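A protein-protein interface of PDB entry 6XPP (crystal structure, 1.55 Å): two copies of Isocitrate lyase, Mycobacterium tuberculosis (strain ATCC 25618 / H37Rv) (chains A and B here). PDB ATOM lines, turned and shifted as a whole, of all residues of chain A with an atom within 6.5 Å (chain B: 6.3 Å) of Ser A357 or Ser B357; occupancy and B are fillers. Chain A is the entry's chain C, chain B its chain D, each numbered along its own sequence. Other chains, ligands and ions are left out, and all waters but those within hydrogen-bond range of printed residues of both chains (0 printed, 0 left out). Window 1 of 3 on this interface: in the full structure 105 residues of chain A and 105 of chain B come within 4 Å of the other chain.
Hydrophobic or aromatic side chains of chain A that line the printed part of chain B: Ala A353, Tyr A356, Phe A359, Leu A376 and Tyr A388.
Printed residues of chain B within 4 Å of Ser A357: Ala B353 (3.4 Å) and Ser B357 (3.2 Å).
Of the printed residues of chain A, Ser B357 touches Ala A353 and Ser A357.
Of the printed residues of chain A, Tyr B388 touches Asn A355, Tyr A356 and Phe A359.
Of the printed residues of chain B, Phe A359 touches Tyr B388.
Printed residues of chain A within 4 Å of Tyr B356: Leu A376 (3.9 Å) and Tyr A388 (3.3 Å).
Of the printed residues of chain B, Tyr A388 touches Asn B355, Tyr B356 and Phe B359.
Leu A354 touches none of the printed residues of chain B.
The nearest residue of chain B that does not touch Ser A357 is Leu B354 (4.4 Å).
The nearest printed residue of chain A that does not touch Leu B376 is His A352 (4.2 Å).
Met B358 touches Ala A353.
Ala A353 touches Leu B376 (N to CD2, 3.97 Å).
Tyr B388 touches Asn A355.
Leu B376 touches Tyr A356 (CD1 to CD2, 3.9 Å).
Tyr B388 touches Phe A359.
Leu A376 touches Ala B353.
Leu A376 touches Tyr B356.
Tyr A388 touches Asn B355.
Tyr A388 touches Phe B359 (CD1 to CG, 3.5 Å).
OG of Ser B357 lies within hydrogen-bond range of O of Ala B353, 2.8 Å away.
The side-chain hydroxyl (OG) of Ser A357 is in hydrogen-bond range of the backbone carbonyl oxygen (O) of Leu A354 (3.2 Å).
The backbone carbonyl oxygen of Ala A353 sits at hydrogen-bond distance from the side-chain hydroxyl of Ser A357, at 2.8 Å.
The side-chain hydroxyl (OG) of Ser B357 lies within hydrogen-bond range of the backbone carbonyl oxygen (O) of Leu B354, at 3.2 Å.
The backbone carbonyl oxygen of Ala B353 is in hydrogen-bond range of the side-chain hydroxyl of Ser A357 (3.4 Å).
OG of Ser B357 is in hydrogen-bond range of O of Ala A353 (3.4 Å).
The side-chain hydroxyl (OH) of Tyr B388 is in hydrogen-bond range of the backbone NH (N) of Tyr A356, at 3.3 Å.
N of Tyr B356 is in hydrogen-bond range of OH of Tyr A388.
The side-chain hydroxyl (OG) of Ser B357 sits at hydrogen-bond distance from the side-chain hydroxyl (OG) of Ser A357, 3.2 Å away.
Ala A353 touches Ser B357, and with the chains exchanged Ser A357 touches Ala B353.
Ala A353 touches Leu B376, and with the chains exchanged Leu A376 touches Ala B353.
Ser B357 touches its own counterpart, Ser A357.
Phe A359 touches Tyr B388, and with the chains exchanged Tyr A388 touches Phe B359.
Of the 14 pairs that touch across the chains among the printed residues, 13 have their exchanged pair printed and touching as well.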
ATOM      1  N   HIS A 352     -28.425  20.716  13.784  1.00  0.00           N
ATOM      2  CA  HIS A 352     -28.426  20.168  12.399  1.00  0.00           C
ATOM      3  C   HIS A 352     -27.003  19.755  11.999  1.00  0.00           C
ATOM      4  O   HIS A 352     -26.837  18.658  11.470  1.00  0.00           O
ATOM      5  CB  HIS A 352     -29.145  21.140  11.458  1.00  0.00           C
ATOM      6  CG  HIS A 352     -30.622  21.085  11.651  1.00  0.00           C
ATOM      7  ND1 HIS A 352     -31.367  19.991  11.261  1.00  0.00           N
ATOM      8  CD2 HIS A 352     -31.489  21.937  12.236  1.00  0.00           C
ATOM      9  CE1 HIS A 352     -32.628  20.185  11.582  1.00  0.00           C
ATOM     10  NE2 HIS A 352     -32.729  21.363  12.195  1.00  0.00           N
ATOM     11  N   ALA A 353     -25.984  20.558  12.286  1.00  0.00           N
ATOM     12  CA  ALA A 353     -24.583  20.227  11.943  1.00  0.00           C
ATOM     13  C   ALA A 353     -24.161  18.939  12.671  1.00  0.00           C
ATOM     14  O   ALA A 353     -23.598  18.045  12.037  1.00  0.00           O
ATOM     15  CB  ALA A 353     -23.664  21.377  12.258  1.00  0.00           C
ATOM     16  N   LEU A 354     -24.452  18.829  13.965  1.00  0.00           N
ATOM     17  CA  LEU A 354     -24.058  17.659  14.796  1.00  0.00           C
ATOM     18  C   LEU A 354     -24.807  16.410  14.330  1.00  0.00           C
ATOM     19  O   LEU A 354     -24.160  15.359  14.144  1.00  0.00           O
ATOM     20  CB  LEU A 354     -24.372  17.963  16.264  1.00  0.00           C
ATOM     21  CG  LEU A 354     -24.022  16.873  17.276  1.00  0.00           C
ATOM     22  CD1 LEU A 354     -23.740  17.498  18.639  1.00  0.00           C
ATOM     23  CD2 LEU A 354     -25.124  15.830  17.391  1.00  0.00           C
ATOM     24  N   ASN A 355     -26.128  16.500  14.187  1.00  0.00           N
ATOM     25  CA  ASN A 355     -26.962  15.318  13.858  1.00  0.00           C
ATOM     26  C   ASN A 355     -26.613  14.858  12.439  1.00  0.00           C
ATOM     27  O   ASN A 355     -26.398  13.656  12.252  1.00  0.00           O
ATOM     28  CB  ASN A 355     -28.452  15.590  14.052  1.00  0.00           C
ATOM     29  CG  ASN A 355     -28.883  15.435  15.499  1.00  0.00           C
ATOM     30  OD1 ASN A 355     -29.253  14.343  15.920  1.00  0.00           O
ATOM     31  ND2 ASN A 355     -28.803  16.505  16.279  1.00  0.00           N
ATOM     32  N   TYR A 356     -26.517  15.774  11.476  1.00  0.00           N
ATOM     33  CA  TYR A 356     -26.245  15.370  10.069  1.00  0.00           C
ATOM     34  C   TYR A 356     -24.847  14.753   9.972  1.00  0.00           C
ATOM     35  O   TYR A 356     -24.700  13.678   9.353  1.00  0.00           O
ATOM     36  CB  TYR A 356     -26.360  16.532   9.083  1.00  0.00           C
ATOM     37  CG  TYR A 356     -25.969  16.085   7.701  1.00  0.00           C
ATOM     38  CD1 TYR A 356     -26.801  15.235   6.999  1.00  0.00           C
ATOM     39  CD2 TYR A 356     -24.727  16.388   7.167  1.00  0.00           C
ATOM     40  CE1 TYR A 356     -26.440  14.748   5.754  1.00  0.00           C
ATOM     41  CE2 TYR A 356     -24.347  15.900   5.925  1.00  0.00           C
ATOM     42  CZ  TYR A 356     -25.216  15.091   5.215  1.00  0.00           C
ATOM     43  OH  TYR A 356     -24.877  14.621   3.977  1.00  0.00           O
ATOM     44  N   SER A 357     -23.827  15.405  10.537  1.00  0.00           N
ATOM     45  CA  SER A 357     -22.421  14.968  10.379  1.00  0.00           C
ATOM     46  C   SER A 357     -22.252  13.577  10.988  1.00  0.00           C
ATOM     47  O   SER A 357     -21.537  12.753  10.393  1.00  0.00           O
ATOM     48  CB  SER A 357     -21.434  15.962  10.936  1.00  0.00           C
ATOM     49  OG  SER A 357     -21.578  16.135  12.337  1.00  0.00           O
ATOM     50  N   MET A 358     -22.875  13.289  12.140  1.00  0.00           N
ATOM     51  CA  MET A 358     -22.706  11.950  12.749  1.00  0.00           C
ATOM     52  C   MET A 358     -23.537  10.926  11.964  1.00  0.00           C
ATOM     53  O   MET A 358     -23.050   9.803  11.797  1.00  0.00           O
ATOM     54  CB  MET A 358     -23.073  11.910  14.236  1.00  0.00           C
ATOM     55  CG  MET A 358     -22.803  10.552  14.866  1.00  0.00           C
ATOM     56  SD  MET A 358     -21.138   9.868  14.586  1.00  0.00           S
ATOM     57  CE  MET A 358     -20.145  11.019  15.534  1.00  0.00           C
ATOM     58  N   PHE A 359     -24.732  11.272  11.498  1.00  0.00           N
ATOM     59  CA  PHE A 359     -25.526  10.336  10.660  1.00  0.00           C
ATOM     60  C   PHE A 359     -24.699   9.972   9.423  1.00  0.00           C
ATOM     61  O   PHE A 359     -24.556   8.779   9.114  1.00  0.00           O
ATOM     62  CB  PHE A 359     -26.879  10.899  10.233  1.00  0.00           C
ATOM     63  CG  PHE A 359     -27.601   9.939   9.322  1.00  0.00           C
ATOM     64  CD1 PHE A 359     -28.336   8.890   9.847  1.00  0.00           C
ATOM     65  CD2 PHE A 359     -27.461  10.031   7.948  1.00  0.00           C
ATOM     66  CE1 PHE A 359     -28.967   7.983   9.010  1.00  0.00           C
ATOM     67  CE2 PHE A 359     -28.087   9.117   7.113  1.00  0.00           C
ATOM     68  CZ  PHE A 359     -28.842   8.102   7.646  1.00  0.00           C
ATOM     69  N   ASP A 360     -24.159  10.981   8.747  1.00  0.00           N
ATOM     70  CA  ASP A 360     -23.402  10.800   7.477  1.00  0.00           C
ATOM     71  C   ASP A 360     -22.195   9.895   7.731  1.00  0.00           C
ATOM     72  O   ASP A 360     -22.009   8.919   6.972  1.00  0.00           O
ATOM     73  CB  ASP A 360     -22.960  12.137   6.889  1.00  0.00           C
ATOM     74  CG  ASP A 360     -22.314  11.984   5.522  1.00  0.00           C
ATOM     75  OD1 ASP A 360     -22.976  11.429   4.644  1.00  0.00           O
ATOM     76  OD2 ASP A 360     -21.149  12.389   5.363  1.00  0.00           O
ATOM     77  N   LEU A 361     -21.407  10.169   8.770  1.00  0.00           N
ATOM     78  CA  LEU A 361     -20.219   9.345   9.100  1.00  0.00           C
ATOM     79  C   LEU A 361     -20.650   7.933   9.497  1.00  0.00           C
ATOM     80  O   LEU A 361     -20.041   6.966   9.002  1.00  0.00           O
ATOM     81  CB  LEU A 361     -19.411  10.000  10.223  1.00  0.00           C
ATOM     82  CG  LEU A 361     -18.227   9.182  10.720  1.00  0.00           C
ATOM     83  CD1 LEU A 361     -17.226   8.889   9.596  1.00  0.00           C
ATOM     84  CD2 LEU A 361     -17.534   9.911  11.863  1.00  0.00           C
ATOM     85  N   ALA A 362     -21.640   7.793  10.380  1.00  0.00           N
ATOM     86  CA  ALA A 362     -22.061   6.477  10.913  1.00  0.00           C
ATOM     87  C   ALA A 362     -22.621   5.608   9.780  1.00  0.00           C
ATOM     88  O   ALA A 362     -22.368   4.402   9.785  1.00  0.00           O
ATOM     89  CB  ALA A 362     -23.067   6.646  12.029  1.00  0.00           C
ATOM     90  N   LEU A 376     -13.516  11.574   5.895  1.00  0.00           N
ATOM     91  CA  LEU A 376     -13.624  12.736   6.814  1.00  0.00           C
ATOM     92  C   LEU A 376     -12.224  13.266   7.125  1.00  0.00           C
ATOM     93  O   LEU A 376     -12.028  14.499   7.027  1.00  0.00           O
ATOM     94  CB  LEU A 376     -14.375  12.326   8.088  1.00  0.00           C
ATOM     95  CG  LEU A 376     -14.399  13.380   9.197  1.00  0.00           C
ATOM     96  CD1 LEU A 376     -15.006  14.684   8.700  1.00  0.00           C
ATOM     97  CD2 LEU A 376     -15.178  12.865  10.389  1.00  0.00           C
ATOM     98  N   TYR A 388      -8.680  25.644   9.397  1.00  0.00           N
ATOM     99  CA  TYR A 388      -9.084  24.541  10.309  1.00  0.00           C
ATOM    100  C   TYR A 388      -7.843  23.979  11.003  1.00  0.00           C
ATOM    101  O   TYR A 388      -6.834  23.735  10.326  1.00  0.00           O
ATOM    102  CB  TYR A 388      -9.818  23.446   9.542  1.00  0.00           C
ATOM    103  CG  TYR A 388     -10.394  22.327  10.375  1.00  0.00           C
ATOM    104  CD1 TYR A 388     -11.469  22.541  11.233  1.00  0.00           C
ATOM    105  CD2 TYR A 388      -9.907  21.038  10.263  1.00  0.00           C
ATOM    106  CE1 TYR A 388     -12.042  21.502  11.951  1.00  0.00           C
ATOM    107  CE2 TYR A 388     -10.464  19.990  10.980  1.00  0.00           C
ATOM    108  CZ  TYR A 388     -11.540  20.218  11.822  1.00  0.00           C
ATOM    109  OH  TYR A 388     -12.070  19.165  12.515  1.00  0.00           O
ATOM    110  N   HIS B 352     -14.185  14.724  15.788  1.00  0.00           N
ATOM    111  CA  HIS B 352     -13.834  15.121  14.400  1.00  0.00           C
ATOM    112  C   HIS B 352     -15.100  15.481  13.621  1.00  0.00           C
ATOM    113  O   HIS B 352     -15.092  16.529  12.941  1.00  0.00           O
ATOM    114  CB  HIS B 352     -12.931  14.056  13.779  1.00  0.00           C
ATOM    115  CG  HIS B 352     -11.541  14.155  14.312  1.00  0.00           C
ATOM    116  ND1 HIS B 352     -10.717  15.219  13.984  1.00  0.00           N
ATOM    117  CD2 HIS B 352     -10.843  13.397  15.185  1.00  0.00           C
ATOM    118  CE1 HIS B 352      -9.565  15.083  14.601  1.00  0.00           C
ATOM    119  NE2 HIS B 352      -9.623  13.986  15.361  1.00  0.00           N
ATOM    120  N   ALA B 353     -16.174  14.702  13.735  1.00  0.00           N
ATOM    121  CA  ALA B 353     -17.446  14.997  13.033  1.00  0.00           C
ATOM    122  C   ALA B 353     -17.983  16.364  13.481  1.00  0.00           C
ATOM    123  O   ALA B 353     -18.336  17.187  12.621  1.00  0.00           O
ATOM    124  CB  ALA B 353     -18.443  13.891  13.255  1.00  0.00           C
ATOM    125  N   LEU B 354     -18.015  16.614  14.792  1.00  0.00           N
ATOM    126  CA  LEU B 354     -18.582  17.858  15.371  1.00  0.00           C
ATOM    127  C   LEU B 354     -17.713  19.056  14.973  1.00  0.00           C
ATOM    128  O   LEU B 354     -18.267  20.075  14.522  1.00  0.00           O
ATOM    129  CB  LEU B 354     -18.654  17.707  16.897  1.00  0.00           C
ATOM    130  CG  LEU B 354     -19.222  18.907  17.662  1.00  0.00           C
ATOM    131  CD1 LEU B 354     -19.842  18.437  18.973  1.00  0.00           C
ATOM    132  CD2 LEU B 354     -18.149  19.951  17.949  1.00  0.00           C
ATOM    133  N   ASN B 355     -16.402  18.957  15.169  1.00  0.00           N
ATOM    134  CA  ASN B 355     -15.487  20.104  14.943  1.00  0.00           C
ATOM    135  C   ASN B 355     -15.458  20.414  13.442  1.00  0.00           C
ATOM    136  O   ASN B 355     -15.594  21.592  13.085  1.00  0.00           O
ATOM    137  CB  ASN B 355     -14.093  19.861  15.524  1.00  0.00           C
ATOM    138  CG  ASN B 355     -14.044  20.163  17.011  1.00  0.00           C
ATOM    139  OD1 ASN B 355     -13.742  21.286  17.398  1.00  0.00           O
ATOM    140  ND2 ASN B 355     -14.344  19.177  17.842  1.00  0.00           N
ATOM    141  N   TYR B 356     -15.339  19.401  12.585  1.00  0.00           N
ATOM    142  CA  TYR B 356     -15.224  19.667  11.130  1.00  0.00           C
ATOM    143  C   TYR B 356     -16.536  20.270  10.608  1.00  0.00           C
ATOM    144  O   TYR B 356     -16.510  21.290   9.872  1.00  0.00           O
ATOM    145  CB  TYR B 356     -14.865  18.426  10.313  1.00  0.00           C
ATOM    146  CG  TYR B 356     -14.832  18.777   8.850  1.00  0.00           C
ATOM    147  CD1 TYR B 356     -13.822  19.588   8.364  1.00  0.00           C
ATOM    148  CD2 TYR B 356     -15.874  18.443   8.002  1.00  0.00           C
ATOM    149  CE1 TYR B 356     -13.801  19.996   7.039  1.00  0.00           C
ATOM    150  CE2 TYR B 356     -15.867  18.838   6.673  1.00  0.00           C
ATOM    151  CZ  TYR B 356     -14.831  19.624   6.198  1.00  0.00           C
ATOM    152  OH  TYR B 356     -14.801  20.043   4.898  1.00  0.00           O
ATOM    153  N   SER B 357     -17.672  19.661  10.955  1.00  0.00           N
ATOM    154  CA  SER B 357     -18.993  20.081  10.421  1.00  0.00           C
ATOM    155  C   SER B 357     -19.285  21.526  10.837  1.00  0.00           C
ATOM    156  O   SER B 357     -19.819  22.277  10.014  1.00  0.00           O
ATOM    157  CB  SER B 357     -20.098  19.135  10.797  1.00  0.00           C
ATOM    158  OG  SER B 357     -20.321  19.101  12.200  1.00  0.00           O
ATOM    159  N   MET B 358     -18.950  21.929  12.066  1.00  0.00           N
ATOM    160  CA  MET B 358     -19.249  23.317  12.489  1.00  0.00           C
ATOM    161  C   MET B 358     -18.240  24.274  11.851  1.00  0.00           C
ATOM    162  O   MET B 358     -18.655  25.376  11.463  1.00  0.00           O
ATOM    163  CB  MET B 358     -19.251  23.510  14.013  1.00  0.00           C
ATOM    164  CG  MET B 358     -19.688  24.908  14.410  1.00  0.00           C
ATOM    165  SD  MET B 358     -21.258  25.471  13.670  1.00  0.00           S
ATOM    166  CE  MET B 358     -22.431  24.361  14.447  1.00  0.00           C
ATOM    167  N   PHE B 359     -16.967  23.892  11.726  1.00  0.00           N
ATOM    168  CA  PHE B 359     -15.991  24.758  11.017  1.00  0.00           C
ATOM    169  C   PHE B 359     -16.495  25.002   9.590  1.00  0.00           C
ATOM    170  O   PHE B 359     -16.550  26.169   9.141  1.00  0.00           O
ATOM    171  CB  PHE B 359     -14.584  24.176  10.972  1.00  0.00           C
ATOM    172  CG  PHE B 359     -13.660  25.067  10.185  1.00  0.00           C
ATOM    173  CD1 PHE B 359     -13.050  26.153  10.783  1.00  0.00           C
ATOM    174  CD2 PHE B 359     -13.460  24.856   8.831  1.00  0.00           C
ATOM    175  CE1 PHE B 359     -12.224  26.995  10.054  1.00  0.00           C
ATOM    176  CE2 PHE B 359     -12.636  25.698   8.103  1.00  0.00           C
ATOM    177  CZ  PHE B 359     -12.007  26.755   8.716  1.00  0.00           C
ATOM    178  N   ASP B 360     -16.869  23.928   8.903  1.00  0.00           N
ATOM    179  CA  ASP B 360     -17.291  23.985   7.478  1.00  0.00           C
ATOM    180  C   ASP B 360     -18.520  24.891   7.341  1.00  0.00           C
ATOM    181  O   ASP B 360     -18.510  25.793   6.470  1.00  0.00           O
ATOM    182  CB  ASP B 360     -17.564  22.585   6.930  1.00  0.00           C
ATOM    183  CG  ASP B 360     -17.859  22.596   5.447  1.00  0.00           C
ATOM    184  OD1 ASP B 360     -17.004  23.105   4.699  1.00  0.00           O
ATOM    185  OD2 ASP B 360     -18.956  22.135   5.076  1.00  0.00           O
ATOM    186  N   LEU B 361     -19.537  24.695   8.181  1.00  0.00           N
ATOM    187  CA  LEU B 361     -20.768  25.526   8.140  1.00  0.00           C
ATOM    188  C   LEU B 361     -20.421  26.979   8.480  1.00  0.00           C
ATOM    189  O   LEU B 361     -20.892  27.885   7.769  1.00  0.00           O
ATOM    190  CB  LEU B 361     -21.814  24.977   9.115  1.00  0.00           C
ATOM    191  CG  LEU B 361     -23.062  25.843   9.277  1.00  0.00           C
ATOM    192  CD1 LEU B 361     -23.792  26.023   7.939  1.00  0.00           C
ATOM    193  CD2 LEU B 361     -23.987  25.233  10.307  1.00  0.00           C
ATOM    194  N   ALA B 362     -19.669  27.221   9.563  1.00  0.00           N
ATOM    195  CA  ALA B 362     -19.407  28.589  10.054  1.00  0.00           C
ATOM    196  C   ALA B 362     -18.583  29.360   9.021  1.00  0.00           C
ATOM    197  O   ALA B 362     -18.833  30.565   8.851  1.00  0.00           O
ATOM    198  CB  ALA B 362     -18.723  28.544  11.395  1.00  0.00           C
ATOM    199  N   LEU B 376     -26.527  22.888   3.762  1.00  0.00           N
ATOM    200  CA  LEU B 376     -26.647  21.827   4.791  1.00  0.00           C
ATOM    201  C   LEU B 376     -28.086  21.304   4.823  1.00  0.00           C
ATOM    202  O   LEU B 376     -28.260  20.069   4.823  1.00  0.00           O
ATOM    203  CB  LEU B 376     -26.211  22.380   6.154  1.00  0.00           C
ATOM    204  CG  LEU B 376     -26.442  21.448   7.343  1.00  0.00           C
ATOM    205  CD1 LEU B 376     -25.759  20.107   7.140  1.00  0.00           C
ATOM    206  CD2 LEU B 376     -25.941  22.093   8.626  1.00  0.00           C
ATOM    207  N   TYR B 388     -32.262   9.152   7.416  1.00  0.00           N
ATOM    208  CA  TYR B 388     -32.088  10.327   8.319  1.00  0.00           C
ATOM    209  C   TYR B 388     -33.457  10.944   8.597  1.00  0.00           C
ATOM    210  O   TYR B 388     -34.254  11.138   7.650  1.00  0.00           O
ATOM    211  CB  TYR B 388     -31.160  11.351   7.677  1.00  0.00           C
ATOM    212  CG  TYR B 388     -30.821  12.572   8.489  1.00  0.00           C
ATOM    213  CD1 TYR B 388     -29.999  12.473   9.592  1.00  0.00           C
ATOM    214  CD2 TYR B 388     -31.245  13.835   8.110  1.00  0.00           C
ATOM    215  CE1 TYR B 388     -29.622  13.598  10.311  1.00  0.00           C
ATOM    216  CE2 TYR B 388     -30.871  14.969   8.813  1.00  0.00           C
ATOM    217  CZ  TYR B 388     -30.057  14.848   9.921  1.00  0.00           C
ATOM    218  OH  TYR B 388     -29.689  15.965  10.624  1.00  0.00           O
